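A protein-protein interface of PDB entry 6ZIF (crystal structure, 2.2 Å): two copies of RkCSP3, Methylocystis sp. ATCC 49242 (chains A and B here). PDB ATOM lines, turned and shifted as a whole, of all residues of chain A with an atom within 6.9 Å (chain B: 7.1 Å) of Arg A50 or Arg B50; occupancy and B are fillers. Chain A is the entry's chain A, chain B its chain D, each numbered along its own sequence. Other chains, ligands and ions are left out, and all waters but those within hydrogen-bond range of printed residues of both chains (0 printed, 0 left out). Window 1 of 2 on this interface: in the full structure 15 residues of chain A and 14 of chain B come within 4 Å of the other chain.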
ATOM      1  N   CYS A  11      13.351  13.037 -20.387  1.00  0.00           N
ATOM      2  CA  CYS A  11      13.092  14.281 -21.110  1.00  0.00           C
ATOM      3  C   CYS A  11      11.891  14.150 -22.071  1.00  0.00           C
ATOM      4  O   CYS A  11      11.085  15.076 -22.204  1.00  0.00           O
ATOM      5  CB  CYS A  11      14.353  14.811 -21.802  1.00  0.00           C
ATOM      6  SG  CYS A  11      15.525  15.673 -20.685  1.00  0.00           S
ATOM      7  N   LEU A  12      11.698  12.978 -22.693  1.00  0.00           N
ATOM      8  CA  LEU A  12      10.529  12.815 -23.559  1.00  0.00           C
ATOM      9  C   LEU A  12       9.244  12.722 -22.748  1.00  0.00           C
ATOM     10  O   LEU A  12       8.224  13.209 -23.189  1.00  0.00           O
ATOM     11  CB  LEU A  12      10.689  11.619 -24.511  1.00  0.00           C
ATOM     12  CG  LEU A  12      11.605  11.902 -25.695  1.00  0.00           C
ATOM     13  CD1 LEU A  12      11.822  10.680 -26.563  1.00  0.00           C
ATOM     14  CD2 LEU A  12      11.127  13.100 -26.503  1.00  0.00           C
ATOM     15  N   CYS A  14       8.762  14.178 -19.854  1.00  0.00           N
ATOM     16  CA  CYS A  14       8.528  15.519 -19.362  1.00  0.00           C
ATOM     17  C   CYS A  14       8.045  16.414 -20.501  1.00  0.00           C
ATOM     18  O   CYS A  14       7.201  17.280 -20.306  1.00  0.00           O
ATOM     19  CB  CYS A  14       9.814  16.062 -18.740  1.00  0.00           C
ATOM     20  SG  CYS A  14       9.460  17.402 -17.590  1.00  0.00           S
ATOM     21  N   TYR A  15       8.586  16.240 -21.700  1.00  0.00           N
ATOM     22  CA  TYR A  15       8.041  16.960 -22.850  1.00  0.00           C
ATOM     23  C   TYR A  15       6.540  16.679 -22.958  1.00  0.00           C
ATOM     24  O   TYR A  15       5.741  17.582 -23.174  1.00  0.00           O
ATOM     25  CB  TYR A  15       8.789  16.612 -24.159  1.00  0.00           C
ATOM     26  CG  TYR A  15       7.934  16.707 -25.397  1.00  0.00           C
ATOM     27  CD1 TYR A  15       7.522  17.940 -25.882  1.00  0.00           C
ATOM     28  CD2 TYR A  15       7.506  15.567 -26.075  1.00  0.00           C
ATOM     29  CE1 TYR A  15       6.699  18.035 -26.998  1.00  0.00           C
ATOM     30  CE2 TYR A  15       6.687  15.656 -27.190  1.00  0.00           C
ATOM     31  CZ  TYR A  15       6.280  16.899 -27.655  1.00  0.00           C
ATOM     32  OH  TYR A  15       5.443  17.029 -28.734  1.00  0.00           O
ATOM     33  N   PHE A  19       3.974  19.798 -22.452  1.00  0.00           N
ATOM     34  CA  PHE A  19       3.327  20.276 -23.670  1.00  0.00           C
ATOM     35  C   PHE A  19       1.868  19.827 -23.717  1.00  0.00           C
ATOM     36  O   PHE A  19       0.989  20.604 -24.082  1.00  0.00           O
ATOM     37  CB  PHE A  19       4.095  19.869 -24.928  1.00  0.00           C
ATOM     38  CG  PHE A  19       3.476  20.432 -26.179  1.00  0.00           C
ATOM     39  CD1 PHE A  19       3.581  21.786 -26.478  1.00  0.00           C
ATOM     40  CD2 PHE A  19       2.763  19.613 -27.049  1.00  0.00           C
ATOM     41  CE1 PHE A  19       2.976  22.301 -27.618  1.00  0.00           C
ATOM     42  CE2 PHE A  19       2.170  20.124 -28.193  1.00  0.00           C
ATOM     43  CZ  PHE A  19       2.281  21.467 -28.474  1.00  0.00           C
ATOM     44  N   SER A  44       8.247  26.650 -22.857  1.00  0.00           N
ATOM     45  CA  SER A  44       9.695  26.722 -22.832  1.00  0.00           C
ATOM     46  C   SER A  44      10.276  25.406 -22.325  1.00  0.00           C
ATOM     47  O   SER A  44      11.151  24.816 -22.955  1.00  0.00           O
ATOM     48  CB  SER A  44      10.078  27.903 -21.964  1.00  0.00           C
ATOM     49  OG  SER A  44      11.451  28.214 -22.014  1.00  0.00           O
ATOM     50  N   CYS A  45       9.803  24.936 -21.171  1.00  0.00           N
ATOM     51  CA  CYS A  45      10.344  23.721 -20.603  1.00  0.00           C
ATOM     52  C   CYS A  45      10.099  22.546 -21.557  1.00  0.00           C
ATOM     53  O   CYS A  45      10.979  21.711 -21.762  1.00  0.00           O
ATOM     54  CB  CYS A  45       9.727  23.435 -19.239  1.00  0.00           C
ATOM     55  SG  CYS A  45      10.529  22.056 -18.372  1.00  0.00           S
ATOM     56  N   ALA A  46       8.907  22.485 -22.160  1.00  0.00           N
ATOM     57  CA  ALA A  46       8.578  21.371 -23.044  1.00  0.00           C
ATOM     58  C   ALA A  46       9.516  21.337 -24.245  1.00  0.00           C
ATOM     59  O   ALA A  46      10.021  20.280 -24.606  1.00  0.00           O
ATOM     60  CB  ALA A  46       7.143  21.470 -23.494  1.00  0.00           C
ATOM     61  N   GLU A  47       9.770  22.507 -24.843  1.00  0.00           N
ATOM     62  CA  GLU A  47      10.692  22.570 -25.953  1.00  0.00           C
ATOM     63  C   GLU A  47      12.117  22.232 -25.524  1.00  0.00           C
ATOM     64  O   GLU A  47      12.831  21.535 -26.241  1.00  0.00           O
ATOM     65  CB  GLU A  47      10.631  23.949 -26.604  1.00  0.00           C
ATOM     66  CG  GLU A  47       9.505  24.112 -27.607  1.00  0.00           C
ATOM     67  CD  GLU A  47       9.279  22.980 -28.609  1.00  0.00           C
ATOM     68  OE1 GLU A  47       8.363  22.188 -28.343  1.00  0.00           O
ATOM     69  OE2 GLU A  47      10.016  22.888 -29.649  1.00  0.00           O
ATOM     70  N   MET A  48      12.551  22.738 -24.358  1.00  0.00           N
ATOM     71  CA  MET A  48      13.887  22.395 -23.895  1.00  0.00           C
ATOM     72  C   MET A  48      14.011  20.888 -23.765  1.00  0.00           C
ATOM     73  O   MET A  48      15.006  20.336 -24.204  1.00  0.00           O
ATOM     74  CB  MET A  48      14.231  23.037 -22.553  1.00  0.00           C
ATOM     75  CG  MET A  48      14.560  24.533 -22.659  1.00  0.00           C
ATOM     76  SD  MET A  48      16.072  24.851 -23.615  1.00  0.00           S
ATOM     77  CE  MET A  48      17.275  24.020 -22.567  1.00  0.00           C
ATOM     78  N   CYS A  49      13.007  20.219 -23.174  1.00  0.00           N
ATOM     79  CA  CYS A  49      13.110  18.783 -22.930  1.00  0.00           C
ATOM     80  C   CYS A  49      13.120  17.998 -24.249  1.00  0.00           C
ATOM     81  O   CYS A  49      13.841  17.012 -24.408  1.00  0.00           O
ATOM     82  CB  CYS A  49      12.025  18.294 -21.979  1.00  0.00           C
ATOM     83  SG  CYS A  49      12.265  18.944 -20.289  1.00  0.00           S
ATOM     84  N   ARG A  50      12.347  18.471 -25.224  1.00  0.00           N
ATOM     85  CA  ARG A  50      12.289  17.825 -26.525  1.00  0.00           C
ATOM     86  C   ARG A  50      13.599  18.080 -27.291  1.00  0.00           C
ATOM     87  O   ARG A  50      14.160  17.185 -27.914  1.00  0.00           O
ATOM     88  CB  ARG A  50      11.016  18.330 -27.199  1.00  0.00           C
ATOM     89  CG  ARG A  50      10.954  18.207 -28.699  1.00  0.00           C
ATOM     90  CD  ARG A  50       9.666  18.909 -29.054  1.00  0.00           C
ATOM     91  NE  ARG A  50       9.229  18.251 -30.254  1.00  0.00           N
ATOM     92  CZ  ARG A  50       8.541  18.825 -31.212  1.00  0.00           C
ATOM     93  NH1 ARG A  50       8.229  20.103 -31.106  1.00  0.00           N
ATOM     94  NH2 ARG A  50       8.190  18.113 -32.271  1.00  0.00           N
ATOM     95  N   ASN A  51      14.138  19.291 -27.175  1.00  0.00           N
ATOM     96  CA  ASN A  51      15.388  19.612 -27.835  1.00  0.00           C
ATOM     97  C   ASN A  51      16.534  18.828 -27.188  1.00  0.00           C
ATOM     98  O   ASN A  51      17.441  18.369 -27.867  1.00  0.00           O
ATOM     99  CB  ASN A  51      15.614  21.118 -27.964  1.00  0.00           C
ATOM    100  CG  ASN A  51      16.972  21.418 -28.569  1.00  0.00           C
ATOM    101  OD1 ASN A  51      17.135  21.313 -29.778  1.00  0.00           O
ATOM    102  ND2 ASN A  51      17.953  21.768 -27.749  1.00  0.00           N
ATOM    103  N   ALA A  52      16.478  18.633 -25.872  1.00  0.00           N
ATOM    104  CA  ALA A  52      17.527  17.900 -25.181  1.00  0.00           C
ATOM    105  C   ALA A  52      17.524  16.445 -25.631  1.00  0.00           C
ATOM    106  O   ALA A  52      18.585  15.852 -25.835  1.00  0.00           O
ATOM    107  CB  ALA A  52      17.352  18.007 -23.706  1.00  0.00           C
ATOM    108  N   ALA A  53      16.329  15.870 -25.791  1.00  0.00           N
ATOM    109  CA  ALA A  53      16.205  14.491 -26.254  1.00  0.00           C
ATOM    110  C   ALA A  53      16.912  14.333 -27.600  1.00  0.00           C
ATOM    111  O   ALA A  53      17.717  13.418 -27.790  1.00  0.00           O
ATOM    112  CB  ALA A  53      14.740  14.081 -26.321  1.00  0.00           C
ATOM    113  N   HIS A  54      16.631  15.262 -28.518  1.00  0.00           N
ATOM    114  CA  HIS A  54      17.162  15.285 -29.858  1.00  0.00           C
ATOM    115  C   HIS A  54      18.692  15.304 -29.832  1.00  0.00           C
ATOM    116  O   HIS A  54      19.345  14.524 -30.539  1.00  0.00           O
ATOM    117  CB  HIS A  54      16.596  16.510 -30.600  1.00  0.00           C
ATOM    118  CG  HIS A  54      16.486  16.345 -32.080  1.00  0.00           C
ATOM    119  ND1 HIS A  54      15.730  15.339 -32.669  1.00  0.00           N
ATOM    120  CD2 HIS A  54      16.995  17.074 -33.098  1.00  0.00           C
ATOM    121  CE1 HIS A  54      15.816  15.437 -33.988  1.00  0.00           C
ATOM    122  NE2 HIS A  54      16.588  16.490 -34.275  1.00  0.00           N
ATOM    123  N   MET A  55      19.261  16.227 -29.042  1.00  0.00           N
ATOM    124  CA  MET A  55      20.703  16.413 -29.002  1.00  0.00           C
ATOM    125  C   MET A  55      21.367  15.164 -28.435  1.00  0.00           C
ATOM    126  O   MET A  55      22.447  14.766 -28.889  1.00  0.00           O
ATOM    127  CB  MET A  55      21.100  17.637 -28.167  1.00  0.00           C
ATOM    128  CG  MET A  55      20.584  18.937 -28.714  1.00  0.00           C
ATOM    129  SD  MET A  55      21.260  19.394 -30.329  1.00  0.00           S
ATOM    130  CE  MET A  55      19.703  19.192 -31.189  1.00  0.00           C
ATOM    131  N   CYS A  70      18.700  22.224 -19.550  1.00  0.00           N
ATOM    132  CA  CYS A  70      17.387  21.631 -19.406  1.00  0.00           C
ATOM    133  C   CYS A  70      17.052  21.447 -17.931  1.00  0.00           C
ATOM    134  O   CYS A  70      15.902  21.569 -17.539  1.00  0.00           O
ATOM    135  CB  CYS A  70      17.261  20.311 -20.150  1.00  0.00           C
ATOM    136  SG  CYS A  70      15.528  19.874 -20.456  1.00  0.00           S
ATOM    137  N   CYS B  11       4.758   6.592 -31.596  1.00  0.00           N
ATOM    138  CA  CYS B  11       5.421   7.562 -32.461  1.00  0.00           C
ATOM    139  C   CYS B  11       6.698   8.130 -31.806  1.00  0.00           C
ATOM    140  O   CYS B  11       7.702   8.341 -32.479  1.00  0.00           O
ATOM    141  CB  CYS B  11       4.438   8.638 -32.938  1.00  0.00           C
ATOM    142  SG  CYS B  11       3.401   8.131 -34.360  1.00  0.00           S
ATOM    143  N   LEU B  12       6.705   8.339 -30.484  1.00  0.00           N
ATOM    144  CA  LEU B  12       7.921   8.835 -29.848  1.00  0.00           C
ATOM    145  C   LEU B  12       8.996   7.751 -29.799  1.00  0.00           C
ATOM    146  O   LEU B  12      10.165   8.050 -29.945  1.00  0.00           O
ATOM    147  CB  LEU B  12       7.643   9.422 -28.454  1.00  0.00           C
ATOM    148  CG  LEU B  12       6.968  10.790 -28.479  1.00  0.00           C
ATOM    149  CD1 LEU B  12       6.602  11.250 -27.079  1.00  0.00           C
ATOM    150  CD2 LEU B  12       7.812  11.834 -29.238  1.00  0.00           C
ATOM    151  N   CYS B  14       9.305   5.340 -31.997  1.00  0.00           N
ATOM    152  CA  CYS B  14       9.750   5.196 -33.360  1.00  0.00           C
ATOM    153  C   CYS B  14      10.617   6.386 -33.768  1.00  0.00           C
ATOM    154  O   CYS B  14      11.597   6.219 -34.480  1.00  0.00           O
ATOM    155  CB  CYS B  14       8.549   5.077 -34.280  1.00  0.00           C
ATOM    156  SG  CYS B  14       8.961   4.273 -35.839  1.00  0.00           S
ATOM    157  N   TYR B  15      10.271   7.585 -33.310  1.00  0.00           N
ATOM    158  CA  TYR B  15      11.157   8.719 -33.524  1.00  0.00           C
ATOM    159  C   TYR B  15      12.545   8.380 -32.970  1.00  0.00           C
ATOM    160  O   TYR B  15      13.568   8.638 -33.608  1.00  0.00           O
ATOM    161  CB  TYR B  15      10.595  10.024 -32.919  1.00  0.00           C
ATOM    162  CG  TYR B  15      11.655  11.002 -32.461  1.00  0.00           C
ATOM    163  CD1 TYR B  15      12.423  11.715 -33.381  1.00  0.00           C
ATOM    164  CD2 TYR B  15      11.904  11.215 -31.108  1.00  0.00           C
ATOM    165  CE1 TYR B  15      13.405  12.606 -32.969  1.00  0.00           C
ATOM    166  CE2 TYR B  15      12.874  12.110 -30.677  1.00  0.00           C
ATOM    167  CZ  TYR B  15      13.633  12.806 -31.611  1.00  0.00           C
ATOM    168  OH  TYR B  15      14.621  13.658 -31.169  1.00  0.00           O
ATOM    169  N   SER B  44      13.265  11.498 -42.551  1.00  0.00           N
ATOM    170  CA  SER B  44      11.899  11.854 -42.876  1.00  0.00           C
ATOM    171  C   SER B  44      10.944  11.142 -41.917  1.00  0.00           C
ATOM    172  O   SER B  44      10.078  11.752 -41.313  1.00  0.00           O
ATOM    173  CB  SER B  44      11.658  11.469 -44.308  1.00  0.00           C
ATOM    174  OG  SER B  44      10.492  12.091 -44.786  1.00  0.00           O
ATOM    175  N   CYS B  45      11.075   9.825 -41.785  1.00  0.00           N
ATOM    176  CA  CYS B  45      10.178   9.077 -40.929  1.00  0.00           C
ATOM    177  C   CYS B  45      10.299   9.569 -39.488  1.00  0.00           C
ATOM    178  O   CYS B  45       9.284   9.719 -38.799  1.00  0.00           O
ATOM    179  CB  CYS B  45      10.475   7.587 -40.995  1.00  0.00           C
ATOM    180  SG  CYS B  45       9.210   6.578 -40.156  1.00  0.00           S
ATOM    181  N   ALA B  46      11.526   9.839 -39.025  1.00  0.00           N
ATOM    182  CA  ALA B  46      11.718  10.270 -37.642  1.00  0.00           C
ATOM    183  C   ALA B  46      11.004  11.587 -37.387  1.00  0.00           C
ATOM    184  O   ALA B  46      10.336  11.741 -36.379  1.00  0.00           O
ATOM    185  CB  ALA B  46      13.196  10.381 -37.307  1.00  0.00           C
ATOM    186  N   GLU B  47      11.120  12.528 -38.316  1.00  0.00           N
ATOM    187  CA  GLU B  47      10.460  13.802 -38.169  1.00  0.00           C
ATOM    188  C   GLU B  47       8.941  13.640 -38.270  1.00  0.00           C
ATOM    189  O   GLU B  47       8.206  14.286 -37.527  1.00  0.00           O
ATOM    190  CB  GLU B  47      10.988  14.778 -39.227  1.00  0.00           C
ATOM    191  CG  GLU B  47      10.705  16.245 -38.904  1.00  0.00           C
ATOM    192  CD  GLU B  47      10.956  16.732 -37.472  1.00  0.00           C
ATOM    193  OE1 GLU B  47      12.053  16.458 -36.884  1.00  0.00           O
ATOM    194  OE2 GLU B  47      10.049  17.392 -36.929  1.00  0.00           O
ATOM    195  N   MET B  48       8.455  12.804 -39.193  1.00  0.00           N
ATOM    196  CA  MET B  48       7.022  12.576 -39.264  1.00  0.00           C
ATOM    197  C   MET B  48       6.513  12.052 -37.919  1.00  0.00           C
ATOM    198  O   MET B  48       5.498  12.539 -37.437  1.00  0.00           O
ATOM    199  CB  MET B  48       6.635  11.560 -40.350  1.00  0.00           C
ATOM    200  CG  MET B  48       6.687  12.116 -41.751  1.00  0.00           C
ATOM    201  SD  MET B  48       5.467  13.402 -42.061  1.00  0.00           S
ATOM    202  CE  MET B  48       3.927  12.545 -41.758  1.00  0.00           C
ATOM    203  N   CYS B  49       7.225  11.092 -37.313  1.00  0.00           N
ATOM    204  CA  CYS B  49       6.746  10.486 -36.074  1.00  0.00           C
ATOM    205  C   CYS B  49       6.762  11.497 -34.928  1.00  0.00           C
ATOM    206  O   CYS B  49       5.857  11.527 -34.084  1.00  0.00           O
ATOM    207  CB  CYS B  49       7.520   9.228 -35.705  1.00  0.00           C
ATOM    208  SG  CYS B  49       7.201   7.860 -36.845  1.00  0.00           S
ATOM    209  N   ARG B  50       7.783  12.360 -34.927  1.00  0.00           N
ATOM    210  CA  ARG B  50       7.906  13.353 -33.880  1.00  0.00           C
ATOM    211  C   ARG B  50       6.853  14.444 -34.081  1.00  0.00           C
ATOM    212  O   ARG B  50       6.221  14.892 -33.127  1.00  0.00           O
ATOM    213  CB  ARG B  50       9.359  13.823 -33.904  1.00  0.00           C
ATOM    214  CG  ARG B  50       9.653  15.024 -33.042  1.00  0.00           C
ATOM    215  CD  ARG B  50      11.024  15.437 -33.529  1.00  0.00           C
ATOM    216  NE  ARG B  50      11.654  16.042 -32.388  1.00  0.00           N
ATOM    217  CZ  ARG B  50      12.500  17.039 -32.457  1.00  0.00           C
ATOM    218  NH1 ARG B  50      12.783  17.552 -33.643  1.00  0.00           N
ATOM    219  NH2 ARG B  50      13.054  17.512 -31.348  1.00  0.00           N
ATOM    220  N   ASN B  51       6.613  14.818 -35.337  1.00  0.00           N
ATOM    221  CA  ASN B  51       5.611  15.821 -35.629  1.00  0.00           C
ATOM    222  C   ASN B  51       4.219  15.283 -35.314  1.00  0.00           C
ATOM    223  O   ASN B  51       3.376  16.009 -34.807  1.00  0.00           O
ATOM    224  CB  ASN B  51       5.772  16.447 -37.016  1.00  0.00           C
ATOM    225  CG  ASN B  51       4.585  17.304 -37.435  1.00  0.00           C
ATOM    226  OD1 ASN B  51       3.736  16.853 -38.183  1.00  0.00           O
ATOM    227  ND2 ASN B  51       4.456  18.525 -36.934  1.00  0.00           N
ATOM    228  N   ALA B  52       3.984  14.001 -35.565  1.00  0.00           N
ATOM    229  CA  ALA B  52       2.686  13.409 -35.285  1.00  0.00           C
ATOM    230  C   ALA B  52       2.434  13.426 -33.785  1.00  0.00           C
ATOM    231  O   ALA B  52       1.322  13.702 -33.350  1.00  0.00           O
ATOM    232  CB  ALA B  52       2.639  11.987 -35.790  1.00  0.00           C
ATOM    233  N   ALA B  53       3.462  13.106 -32.988  1.00  0.00           N
ATOM    234  CA  ALA B  53       3.317  13.092 -31.534  1.00  0.00           C
ATOM    235  C   ALA B  53       2.861  14.469 -31.047  1.00  0.00           C
ATOM    236  O   ALA B  53       1.907  14.590 -30.298  1.00  0.00           O
ATOM    237  CB  ALA B  53       4.609  12.658 -30.890  1.00  0.00           C
ATOM    238  N   HIS B  54       3.521  15.509 -31.552  1.00  0.00           N
ATOM    239  CA  HIS B  54       3.249  16.892 -31.219  1.00  0.00           C
ATOM    240  C   HIS B  54       1.791  17.255 -31.529  1.00  0.00           C
ATOM    241  O   HIS B  54       1.108  17.834 -30.698  1.00  0.00           O
ATOM    242  CB  HIS B  54       4.230  17.777 -32.005  1.00  0.00           C
ATOM    243  CG  HIS B  54       4.552  19.068 -31.344  1.00  0.00           C
ATOM    244  ND1 HIS B  54       5.199  19.115 -30.128  1.00  0.00           N
ATOM    245  CD2 HIS B  54       4.398  20.354 -31.742  1.00  0.00           C
ATOM    246  CE1 HIS B  54       5.422  20.377 -29.795  1.00  0.00           C
ATOM    247  NE2 HIS B  54       4.925  21.159 -30.758  1.00  0.00           N
ATOM    248  N   MET B  55       1.337  16.952 -32.755  1.00  0.00           N
ATOM    249  CA  MET B  55       0.002  17.319 -33.200  1.00  0.00           C
ATOM    250  C   MET B  55      -1.040  16.572 -32.364  1.00  0.00           C
ATOM    251  O   MET B  55      -2.089  17.120 -32.045  1.00  0.00           O
ATOM    252  CB  MET B  55      -0.205  16.989 -34.679  1.00  0.00           C
ATOM    253  CG  MET B  55       0.713  17.773 -35.620  1.00  0.00           C
ATOM    254  SD  MET B  55       0.351  19.538 -35.648  1.00  0.00           S
ATOM    255  CE  MET B  55       1.535  20.164 -34.455  1.00  0.00           C
ATOM    256  N   MET B  56      -0.751  15.323 -31.986  1.00  0.00           N
ATOM    257  CA  MET B  56      -1.657  14.579 -31.130  1.00  0.00           C
ATOM    258  C   MET B  56      -1.700  15.183 -29.730  1.00  0.00           C
ATOM    259  O   MET B  56      -2.775  15.323 -29.158  1.00  0.00           O
ATOM    260  CB  MET B  56      -1.237  13.112 -31.027  1.00  0.00           C
ATOM    261  CG  MET B  56      -1.624  12.282 -32.266  1.00  0.00           C
ATOM    262  SD  MET B  56      -1.163  10.518 -32.039  1.00  0.00           S
ATOM    263  CE  MET B  56       0.616  10.560 -32.286  1.00  0.00           C
ATOM    264  N   LEU B  57      -0.528  15.537 -29.171  1.00  0.00           N
ATOM    265  CA  LEU B  57      -0.456  16.015 -27.799  1.00  0.00           C
ATOM    266  C   LEU B  57      -1.253  17.302 -27.626  1.00  0.00           C
ATOM    267  O   LEU B  57      -1.733  17.564 -26.535  1.00  0.00           O
ATOM    268  CB  LEU B  57       1.008  16.249 -27.406  1.00  0.00           C
ATOM    269  CG  LEU B  57       1.762  14.999 -26.957  1.00  0.00           C
ATOM    270  CD1 LEU B  57       3.255  15.275 -26.903  1.00  0.00           C
ATOM    271  CD2 LEU B  57       1.228  14.485 -25.617  1.00  0.00           C
ATOM    272  N   CYS B  70       1.690   9.557 -41.338  1.00  0.00           N
ATOM    273  CA  CYS B  70       2.781   8.957 -40.598  1.00  0.00           C
ATOM    274  C   CYS B  70       2.799   7.447 -40.830  1.00  0.00           C
ATOM    275  O   CYS B  70       3.868   6.850 -40.870  1.00  0.00           O
ATOM    276  CB  CYS B  70       2.709   9.256 -39.108  1.00  0.00           C
ATOM    277  SG  CYS B  70       4.315   9.004 -38.300  1.00  0.00           S
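Leu B57 touches Tyr A15 (CD1 to OH, 3.3 Å).
Phe A19 touches His B54 (CZ to NE2, 3.5 Å).
CB of Leu B57 touches CD2 of Phe A19, at 3.8 Å.
Glu A47 touches His B54.
CG of Arg A50 touches NH2 of Arg B50, at 3.5 Å.
ND1 of His A54 touches CZ of Arg B50, at 3.7 Å.
Arg A50 touches just these residues of chain B: Arg B50 and His B54.
Of chain A, only Arg A50 (3.5 Å) and His A54 (3.7 Å) come within 4 Å of Arg B50.
Of the printed residues of chain A, Leu B57 touches Tyr A15 (3.3 Å) and Phe A19 (3.8 Å).
Printed residues of chain B within 4 Å of Phe A19: His B54 and Leu B57.
Of the printed residues of chain A, His B54 touches Tyr A15, Phe A19, Glu A47 and Arg A50.
Printed residues of chain B within 4 Å of Tyr A15: His B54 and Leu B57.
Cys A70 touches none of the printed residues of chain B.
Cys B14 touches none of the printed residues of chain A.
The nearest printed residue of chain B that does not touch Phe A19 is Met B55 (5.6 Å).
The side-chain carboxylate of Glu A47 lies within salt-bridge range of the guanidinium group of Arg A50.
The side-chain carboxylate of Glu B47 is in salt-bridge range of the guanidinium group of Arg B50, at 3.5 Å.
Printed residues of chain A that touch a printed residue of chain B: Tyr A15, Phe A19, Glu A47, Arg A50 and His A54.
Hydrophobic or aromatic side chains of chain A within 4 Å of the printed part of chain B: Tyr A15, Phe A19 and His A54.
Of the 19 printed residues of chain B, 4 touch a printed residue of chain A.
Hydrophobic or aromatic side chains of chain B within 4 Å of the printed part of chain A: Tyr B15, His B54 and Leu B57.
Tyr A15 touches His B54, and with the chains exchanged His A54 touches Tyr B15.
Glu A47 touches His B54, but with the chains exchanged His A54 does not touch Glu B47 (4.9 Å).
Arg A50 touches its own counterpart, Arg B50.
Arg A50 touches His B54, and with the chains exchanged His A54 touches Arg B50.
The side-chain hydroxyl (OH) of Tyr A15 sits at hydrogen-bond distance from a ring nitrogen (ND1) of His B54 (2.5 Å).
The guanidinium group (NH1) of Arg A50 sits close to a ring nitrogen (ND1) of His B54 (3.3 Å).
ND1 of His A54 lies within hydrogen-bond range of OH of Tyr B15.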
